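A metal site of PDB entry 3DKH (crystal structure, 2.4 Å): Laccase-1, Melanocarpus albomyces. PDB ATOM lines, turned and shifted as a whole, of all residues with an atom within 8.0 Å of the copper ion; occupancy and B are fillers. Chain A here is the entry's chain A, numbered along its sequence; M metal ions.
A ring nitrogen (NE2) of His 431 lies within hydrogen-bond range of the backbone carbonyl oxygen (O) of Leu 429, 3.4 Å away.
The backbone NH (N) of Leu 481 sits at hydrogen-bond distance from the backbone carbonyl oxygen (O) of His 431, 2.7 Å away.
N of Cys 503 is in hydrogen-bond range of O of Leu 513.
The side-chain sulfur of Cys 503 sits close to the backbone NH of Ile 505 (3.5 Å).
The backbone NH (N) of Leu 513 is in hydrogen-bond range of the backbone carbonyl oxygen (O) of His 508, at 3.0 Å.
CD1 of Ile 505 touches the copper ion, 3.8 Å away.
CD1 of Leu 513 touches the copper ion, 3.7 Å away.
The nearest printed residue that does not touch the copper ion is Pro 430 (4.3 Å).
The copper ion is bound by a ring nitrogen (ND1) of His 431, the side-chain sulfur (SG) of Cys 503 and a ring nitrogen (ND1) of His 508.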
ATOM      1  N   GLU A 235      -2.678 -28.416   0.886  1.00  0.00           N
ATOM      2  CA  GLU A 235      -3.799 -28.000   0.025  1.00  0.00           C
ATOM      3  C   GLU A 235      -5.023 -27.596   0.826  1.00  0.00           C
ATOM      4  O   GLU A 235      -5.645 -26.586   0.523  1.00  0.00           O
ATOM      5  CB  GLU A 235      -4.185 -29.106  -0.976  1.00  0.00           C
ATOM      6  CG  GLU A 235      -5.165 -28.697  -2.102  1.00  0.00           C
ATOM      7  CD  GLU A 235      -6.657 -28.856  -1.770  1.00  0.00           C
ATOM      8  OE1 GLU A 235      -6.993 -29.666  -0.882  1.00  0.00           O
ATOM      9  OE2 GLU A 235      -7.478 -28.157  -2.386  1.00  0.00           O
ATOM     10  N   HIS A 237      -7.810 -26.110   3.195  1.00  0.00           N
ATOM     11  CA  HIS A 237      -8.110 -24.828   3.826  1.00  0.00           C
ATOM     12  C   HIS A 237      -9.229 -25.128   4.829  1.00  0.00           C
ATOM     13  O   HIS A 237     -10.291 -25.660   4.469  1.00  0.00           O
ATOM     14  CB  HIS A 237      -8.600 -23.811   2.832  1.00  0.00           C
ATOM     15  CG  HIS A 237      -7.624 -23.489   1.755  1.00  0.00           C
ATOM     16  ND1 HIS A 237      -7.204 -24.416   0.828  1.00  0.00           N
ATOM     17  CD2 HIS A 237      -7.028 -22.326   1.411  1.00  0.00           C
ATOM     18  CE1 HIS A 237      -6.404 -23.831  -0.042  1.00  0.00           C
ATOM     19  NE2 HIS A 237      -6.283 -22.560   0.294  1.00  0.00           N
ATOM     20  N   VAL A 361      -3.119 -14.587 -13.265  1.00  0.00           N
ATOM     21  CA  VAL A 361      -2.957 -16.007 -12.981  1.00  0.00           C
ATOM     22  C   VAL A 361      -3.797 -16.740 -14.026  1.00  0.00           C
ATOM     23  O   VAL A 361      -4.973 -16.436 -14.204  1.00  0.00           O
ATOM     24  CB  VAL A 361      -3.462 -16.365 -11.552  1.00  0.00           C
ATOM     25  CG1 VAL A 361      -3.373 -17.858 -11.297  1.00  0.00           C
ATOM     26  CG2 VAL A 361      -2.660 -15.614 -10.519  1.00  0.00           C
ATOM     27  N   TRP A 373       0.311 -24.024 -14.042  1.00  0.00           N
ATOM     28  CA  TRP A 373      -0.137 -22.709 -13.570  1.00  0.00           C
ATOM     29  C   TRP A 373       0.799 -21.574 -13.989  1.00  0.00           C
ATOM     30  O   TRP A 373       1.973 -21.582 -13.653  1.00  0.00           O
ATOM     31  CB  TRP A 373      -0.311 -22.735 -12.053  1.00  0.00           C
ATOM     32  CG  TRP A 373      -1.446 -23.595 -11.614  1.00  0.00           C
ATOM     33  CD1 TRP A 373      -1.371 -24.899 -11.225  1.00  0.00           C
ATOM     34  CD2 TRP A 373      -2.825 -23.238 -11.566  1.00  0.00           C
ATOM     35  NE1 TRP A 373      -2.624 -25.382 -10.945  1.00  0.00           N
ATOM     36  CE2 TRP A 373      -3.545 -24.389 -11.145  1.00  0.00           C
ATOM     37  CE3 TRP A 373      -3.544 -22.047 -11.843  1.00  0.00           C
ATOM     38  CZ2 TRP A 373      -4.955 -24.393 -10.993  1.00  0.00           C
ATOM     39  CZ3 TRP A 373      -4.954 -22.052 -11.691  1.00  0.00           C
ATOM     40  CH2 TRP A 373      -5.638 -23.224 -11.271  1.00  0.00           C
ATOM     41  N   ASN A 421      -7.436 -13.585 -11.105  1.00  0.00           N
ATOM     42  CA  ASN A 421      -7.654 -15.043 -11.058  1.00  0.00           C
ATOM     43  C   ASN A 421      -8.359 -15.684 -12.260  1.00  0.00           C
ATOM     44  O   ASN A 421      -9.506 -16.118 -12.140  1.00  0.00           O
ATOM     45  CB  ASN A 421      -8.426 -15.405  -9.787  1.00  0.00           C
ATOM     46  CG  ASN A 421      -8.180 -16.834  -9.337  1.00  0.00           C
ATOM     47  OD1 ASN A 421      -7.545 -17.636 -10.026  1.00  0.00           O
ATOM     48  ND2 ASN A 421      -8.674 -17.159  -8.148  1.00  0.00           N
ATOM     49  N   LEU A 429     -10.164 -21.583  -9.535  1.00  0.00           N
ATOM     50  CA  LEU A 429     -10.077 -22.078  -8.167  1.00  0.00           C
ATOM     51  C   LEU A 429      -9.508 -21.008  -7.241  1.00  0.00           C
ATOM     52  O   LEU A 429      -8.780 -20.122  -7.703  1.00  0.00           O
ATOM     53  CB  LEU A 429      -9.164 -23.322  -8.145  1.00  0.00           C
ATOM     54  CG  LEU A 429      -9.684 -24.646  -8.714  1.00  0.00           C
ATOM     55  CD1 LEU A 429      -8.524 -25.620  -8.885  1.00  0.00           C
ATOM     56  CD2 LEU A 429     -10.739 -25.248  -7.797  1.00  0.00           C
ATOM     57  N   PRO A 430      -9.864 -21.034  -5.926  1.00  0.00           N
ATOM     58  CA  PRO A 430      -9.353 -20.048  -4.962  1.00  0.00           C
ATOM     59  C   PRO A 430      -7.855 -20.280  -4.689  1.00  0.00           C
ATOM     60  O   PRO A 430      -7.391 -21.430  -4.670  1.00  0.00           O
ATOM     61  CB  PRO A 430     -10.186 -20.337  -3.707  1.00  0.00           C
ATOM     62  CG  PRO A 430     -11.434 -20.904  -4.235  1.00  0.00           C
ATOM     63  CD  PRO A 430     -10.922 -21.844  -5.293  1.00  0.00           C
ATOM     64  N   HIS A 431      -7.095 -19.191  -4.524  1.00  0.00           N
ATOM     65  CA  HIS A 431      -5.649 -19.301  -4.300  1.00  0.00           C
ATOM     66  C   HIS A 431      -5.114 -18.558  -3.076  1.00  0.00           C
ATOM     67  O   HIS A 431      -5.240 -17.342  -3.002  1.00  0.00           O
ATOM     68  CB  HIS A 431      -4.850 -18.825  -5.537  1.00  0.00           C
ATOM     69  CG  HIS A 431      -5.109 -19.617  -6.793  1.00  0.00           C
ATOM     70  ND1 HIS A 431      -5.043 -20.984  -6.837  1.00  0.00           N
ATOM     71  CD2 HIS A 431      -5.434 -19.212  -8.042  1.00  0.00           C
ATOM     72  CE1 HIS A 431      -5.319 -21.397  -8.063  1.00  0.00           C
ATOM     73  NE2 HIS A 431      -5.556 -20.340  -8.815  1.00  0.00           N
ATOM     74  N   PRO A 432      -4.533 -19.278  -2.090  1.00  0.00           N
ATOM     75  CA  PRO A 432      -3.964 -18.650  -0.898  1.00  0.00           C
ATOM     76  C   PRO A 432      -2.621 -18.004  -1.250  1.00  0.00           C
ATOM     77  O   PRO A 432      -1.593 -18.669  -1.304  1.00  0.00           O
ATOM     78  CB  PRO A 432      -3.830 -19.829   0.067  1.00  0.00           C
ATOM     79  CG  PRO A 432      -3.575 -20.988  -0.842  1.00  0.00           C
ATOM     80  CD  PRO A 432      -4.571 -20.749  -1.934  1.00  0.00           C
ATOM     81  N   MET A 433      -2.664 -16.739  -1.618  1.00  0.00           N
ATOM     82  CA  MET A 433      -1.455 -16.013  -1.995  1.00  0.00           C
ATOM     83  C   MET A 433      -0.591 -15.624  -0.802  1.00  0.00           C
ATOM     84  O   MET A 433      -1.055 -15.044   0.174  1.00  0.00           O
ATOM     85  CB  MET A 433      -1.801 -14.800  -2.854  1.00  0.00           C
ATOM     86  CG  MET A 433      -2.447 -15.163  -4.186  1.00  0.00           C
ATOM     87  SD  MET A 433      -1.613 -16.449  -5.141  1.00  0.00           S
ATOM     88  CE  MET A 433      -0.415 -15.525  -6.023  1.00  0.00           C
ATOM     89  N   MET A 480      -6.424 -14.830   0.664  1.00  0.00           N
ATOM     90  CA  MET A 480      -7.078 -15.490  -0.460  1.00  0.00           C
ATOM     91  C   MET A 480      -7.309 -14.681  -1.720  1.00  0.00           C
ATOM     92  O   MET A 480      -7.808 -13.559  -1.676  1.00  0.00           O
ATOM     93  CB  MET A 480      -8.421 -16.087  -0.040  1.00  0.00           C
ATOM     94  CG  MET A 480      -8.340 -17.222   0.960  1.00  0.00           C
ATOM     95  SD  MET A 480      -7.259 -18.540   0.445  1.00  0.00           S
ATOM     96  CE  MET A 480      -8.255 -19.342  -0.770  1.00  0.00           C
ATOM     97  N   LEU A 481      -6.935 -15.274  -2.854  1.00  0.00           N
ATOM     98  CA  LEU A 481      -7.199 -14.691  -4.158  1.00  0.00           C
ATOM     99  C   LEU A 481      -8.473 -15.459  -4.503  1.00  0.00           C
ATOM    100  O   LEU A 481      -8.453 -16.686  -4.664  1.00  0.00           O
ATOM    101  CB  LEU A 481      -6.069 -14.976  -5.149  1.00  0.00           C
ATOM    102  CG  LEU A 481      -6.261 -14.784  -6.657  1.00  0.00           C
ATOM    103  CD1 LEU A 481      -6.526 -13.359  -7.048  1.00  0.00           C
ATOM    104  CD2 LEU A 481      -5.061 -15.321  -7.396  1.00  0.00           C
ATOM    105  N   HIS A 502       3.867 -16.523  -4.116  1.00  0.00           N
ATOM    106  CA  HIS A 502       3.242 -17.685  -4.675  1.00  0.00           C
ATOM    107  C   HIS A 502       1.996 -18.173  -3.970  1.00  0.00           C
ATOM    108  O   HIS A 502       1.696 -17.761  -2.842  1.00  0.00           O
ATOM    109  CB  HIS A 502       4.269 -18.840  -4.706  1.00  0.00           C
ATOM    110  CG  HIS A 502       4.653 -19.364  -3.357  1.00  0.00           C
ATOM    111  ND1 HIS A 502       4.095 -20.500  -2.818  1.00  0.00           N
ATOM    112  CD2 HIS A 502       5.536 -18.895  -2.437  1.00  0.00           C
ATOM    113  CE1 HIS A 502       4.617 -20.726  -1.623  1.00  0.00           C
ATOM    114  NE2 HIS A 502       5.495 -19.762  -1.370  1.00  0.00           N
ATOM    115  N   CYS A 503       1.330 -19.114  -4.634  1.00  0.00           N
ATOM    116  CA  CYS A 503       0.153 -19.768  -4.090  1.00  0.00           C
ATOM    117  C   CYS A 503       0.764 -20.805  -3.163  1.00  0.00           C
ATOM    118  O   CYS A 503       1.754 -21.469  -3.520  1.00  0.00           O
ATOM    119  CB  CYS A 503      -0.630 -20.484  -5.183  1.00  0.00           C
ATOM    120  SG  CYS A 503      -1.981 -21.428  -4.495  1.00  0.00           S
ATOM    121  N   HIS A 504       0.193 -20.926  -1.959  1.00  0.00           N
ATOM    122  CA  HIS A 504       0.710 -21.877  -1.000  1.00  0.00           C
ATOM    123  C   HIS A 504       0.175 -23.316  -1.083  1.00  0.00           C
ATOM    124  O   HIS A 504       0.572 -24.174  -0.292  1.00  0.00           O
ATOM    125  CB  HIS A 504       0.674 -21.305   0.406  1.00  0.00           C
ATOM    126  CG  HIS A 504       1.828 -21.746   1.253  1.00  0.00           C
ATOM    127  ND1 HIS A 504       2.020 -23.062   1.619  1.00  0.00           N
ATOM    128  CD2 HIS A 504       2.867 -21.055   1.766  1.00  0.00           C
ATOM    129  CE1 HIS A 504       3.124 -23.165   2.326  1.00  0.00           C
ATOM    130  NE2 HIS A 504       3.655 -21.959   2.430  1.00  0.00           N
ATOM    131  N   ILE A 505      -0.738 -23.576  -2.032  1.00  0.00           N
ATOM    132  CA  ILE A 505      -1.215 -24.948  -2.270  1.00  0.00           C
ATOM    133  C   ILE A 505       0.025 -25.556  -2.959  1.00  0.00           C
ATOM    134  O   ILE A 505       0.490 -25.027  -3.978  1.00  0.00           O
ATOM    135  CB  ILE A 505      -2.448 -25.019  -3.221  1.00  0.00           C
ATOM    136  CG1 ILE A 505      -3.713 -24.629  -2.467  1.00  0.00           C
ATOM    137  CG2 ILE A 505      -2.606 -26.441  -3.826  1.00  0.00           C
ATOM    138  CD1 ILE A 505      -4.931 -24.334  -3.345  1.00  0.00           C
ATOM    139  N   ALA A 506       0.614 -26.557  -2.303  1.00  0.00           N
ATOM    140  CA  ALA A 506       1.829 -27.237  -2.759  1.00  0.00           C
ATOM    141  C   ALA A 506       1.819 -27.652  -4.211  1.00  0.00           C
ATOM    142  O   ALA A 506       2.767 -27.374  -4.942  1.00  0.00           O
ATOM    143  CB  ALA A 506       2.131 -28.419  -1.891  1.00  0.00           C
ATOM    144  N   TRP A 507       0.688 -28.200  -4.634  1.00  0.00           N
ATOM    145  CA  TRP A 507       0.498 -28.674  -6.004  1.00  0.00           C
ATOM    146  C   TRP A 507       0.486 -27.546  -7.034  1.00  0.00           C
ATOM    147  O   TRP A 507       0.999 -27.704  -8.153  1.00  0.00           O
ATOM    148  CB  TRP A 507      -0.783 -29.498  -6.119  1.00  0.00           C
ATOM    149  CG  TRP A 507      -1.254 -30.275  -4.870  1.00  0.00           C
ATOM    150  CD1 TRP A 507      -2.539 -30.316  -4.409  1.00  0.00           C
ATOM    151  CD2 TRP A 507      -0.479 -31.089  -3.950  1.00  0.00           C
ATOM    152  NE1 TRP A 507      -2.631 -31.089  -3.285  1.00  0.00           N
ATOM    153  CE2 TRP A 507      -1.391 -31.575  -2.966  1.00  0.00           C
ATOM    154  CE3 TRP A 507       0.888 -31.451  -3.865  1.00  0.00           C
ATOM    155  CZ2 TRP A 507      -0.970 -32.401  -1.895  1.00  0.00           C
ATOM    156  CZ3 TRP A 507       1.305 -32.268  -2.796  1.00  0.00           C
ATOM    157  CH2 TRP A 507       0.367 -32.742  -1.817  1.00  0.00           C
ATOM    158  N   HIS A 508      -0.043 -26.393  -6.637  1.00  0.00           N
ATOM    159  CA  HIS A 508      -0.124 -25.228  -7.511  1.00  0.00           C
ATOM    160  C   HIS A 508       1.195 -24.491  -7.718  1.00  0.00           C
ATOM    161  O   HIS A 508       1.505 -24.094  -8.858  1.00  0.00           O
ATOM    162  CB  HIS A 508      -1.254 -24.287  -7.064  1.00  0.00           C
ATOM    163  CG  HIS A 508      -2.625 -24.890  -7.174  1.00  0.00           C
ATOM    164  ND1 HIS A 508      -3.746 -24.269  -6.683  1.00  0.00           N
ATOM    165  CD2 HIS A 508      -3.047 -26.059  -7.716  1.00  0.00           C
ATOM    166  CE1 HIS A 508      -4.805 -25.028  -6.914  1.00  0.00           C
ATOM    167  NE2 HIS A 508      -4.407 -26.117  -7.543  1.00  0.00           N
ATOM    168  N   VAL A 509       1.996 -24.361  -6.667  1.00  0.00           N
ATOM    169  CA  VAL A 509       3.318 -23.715  -6.764  1.00  0.00           C
ATOM    170  C   VAL A 509       4.247 -24.643  -7.563  1.00  0.00           C
ATOM    171  O   VAL A 509       5.137 -24.176  -8.279  1.00  0.00           O
ATOM    172  CB  VAL A 509       3.909 -23.289  -5.363  1.00  0.00           C
ATOM    173  CG1 VAL A 509       4.157 -24.479  -4.458  1.00  0.00           C
ATOM    174  CG2 VAL A 509       5.175 -22.466  -5.547  1.00  0.00           C
ATOM    175  N   LEU A 513       2.618 -21.644 -10.181  1.00  0.00           N
ATOM    176  CA  LEU A 513       2.002 -20.439  -9.629  1.00  0.00           C
ATOM    177  C   LEU A 513       2.903 -19.684  -8.665  1.00  0.00           C
ATOM    178  O   LEU A 513       2.766 -19.811  -7.436  1.00  0.00           O
ATOM    179  CB  LEU A 513       0.662 -20.750  -8.966  1.00  0.00           C
ATOM    180  CG  LEU A 513      -0.515 -19.821  -9.316  1.00  0.00           C
ATOM    181  CD1 LEU A 513      -1.791 -20.554  -9.013  1.00  0.00           C
ATOM    182  CD2 LEU A 513      -0.458 -18.493  -8.567  1.00  0.00           C
HETATM  183 CU    CU M   1      -3.377 -22.113  -6.036  1.00  0.00          CU
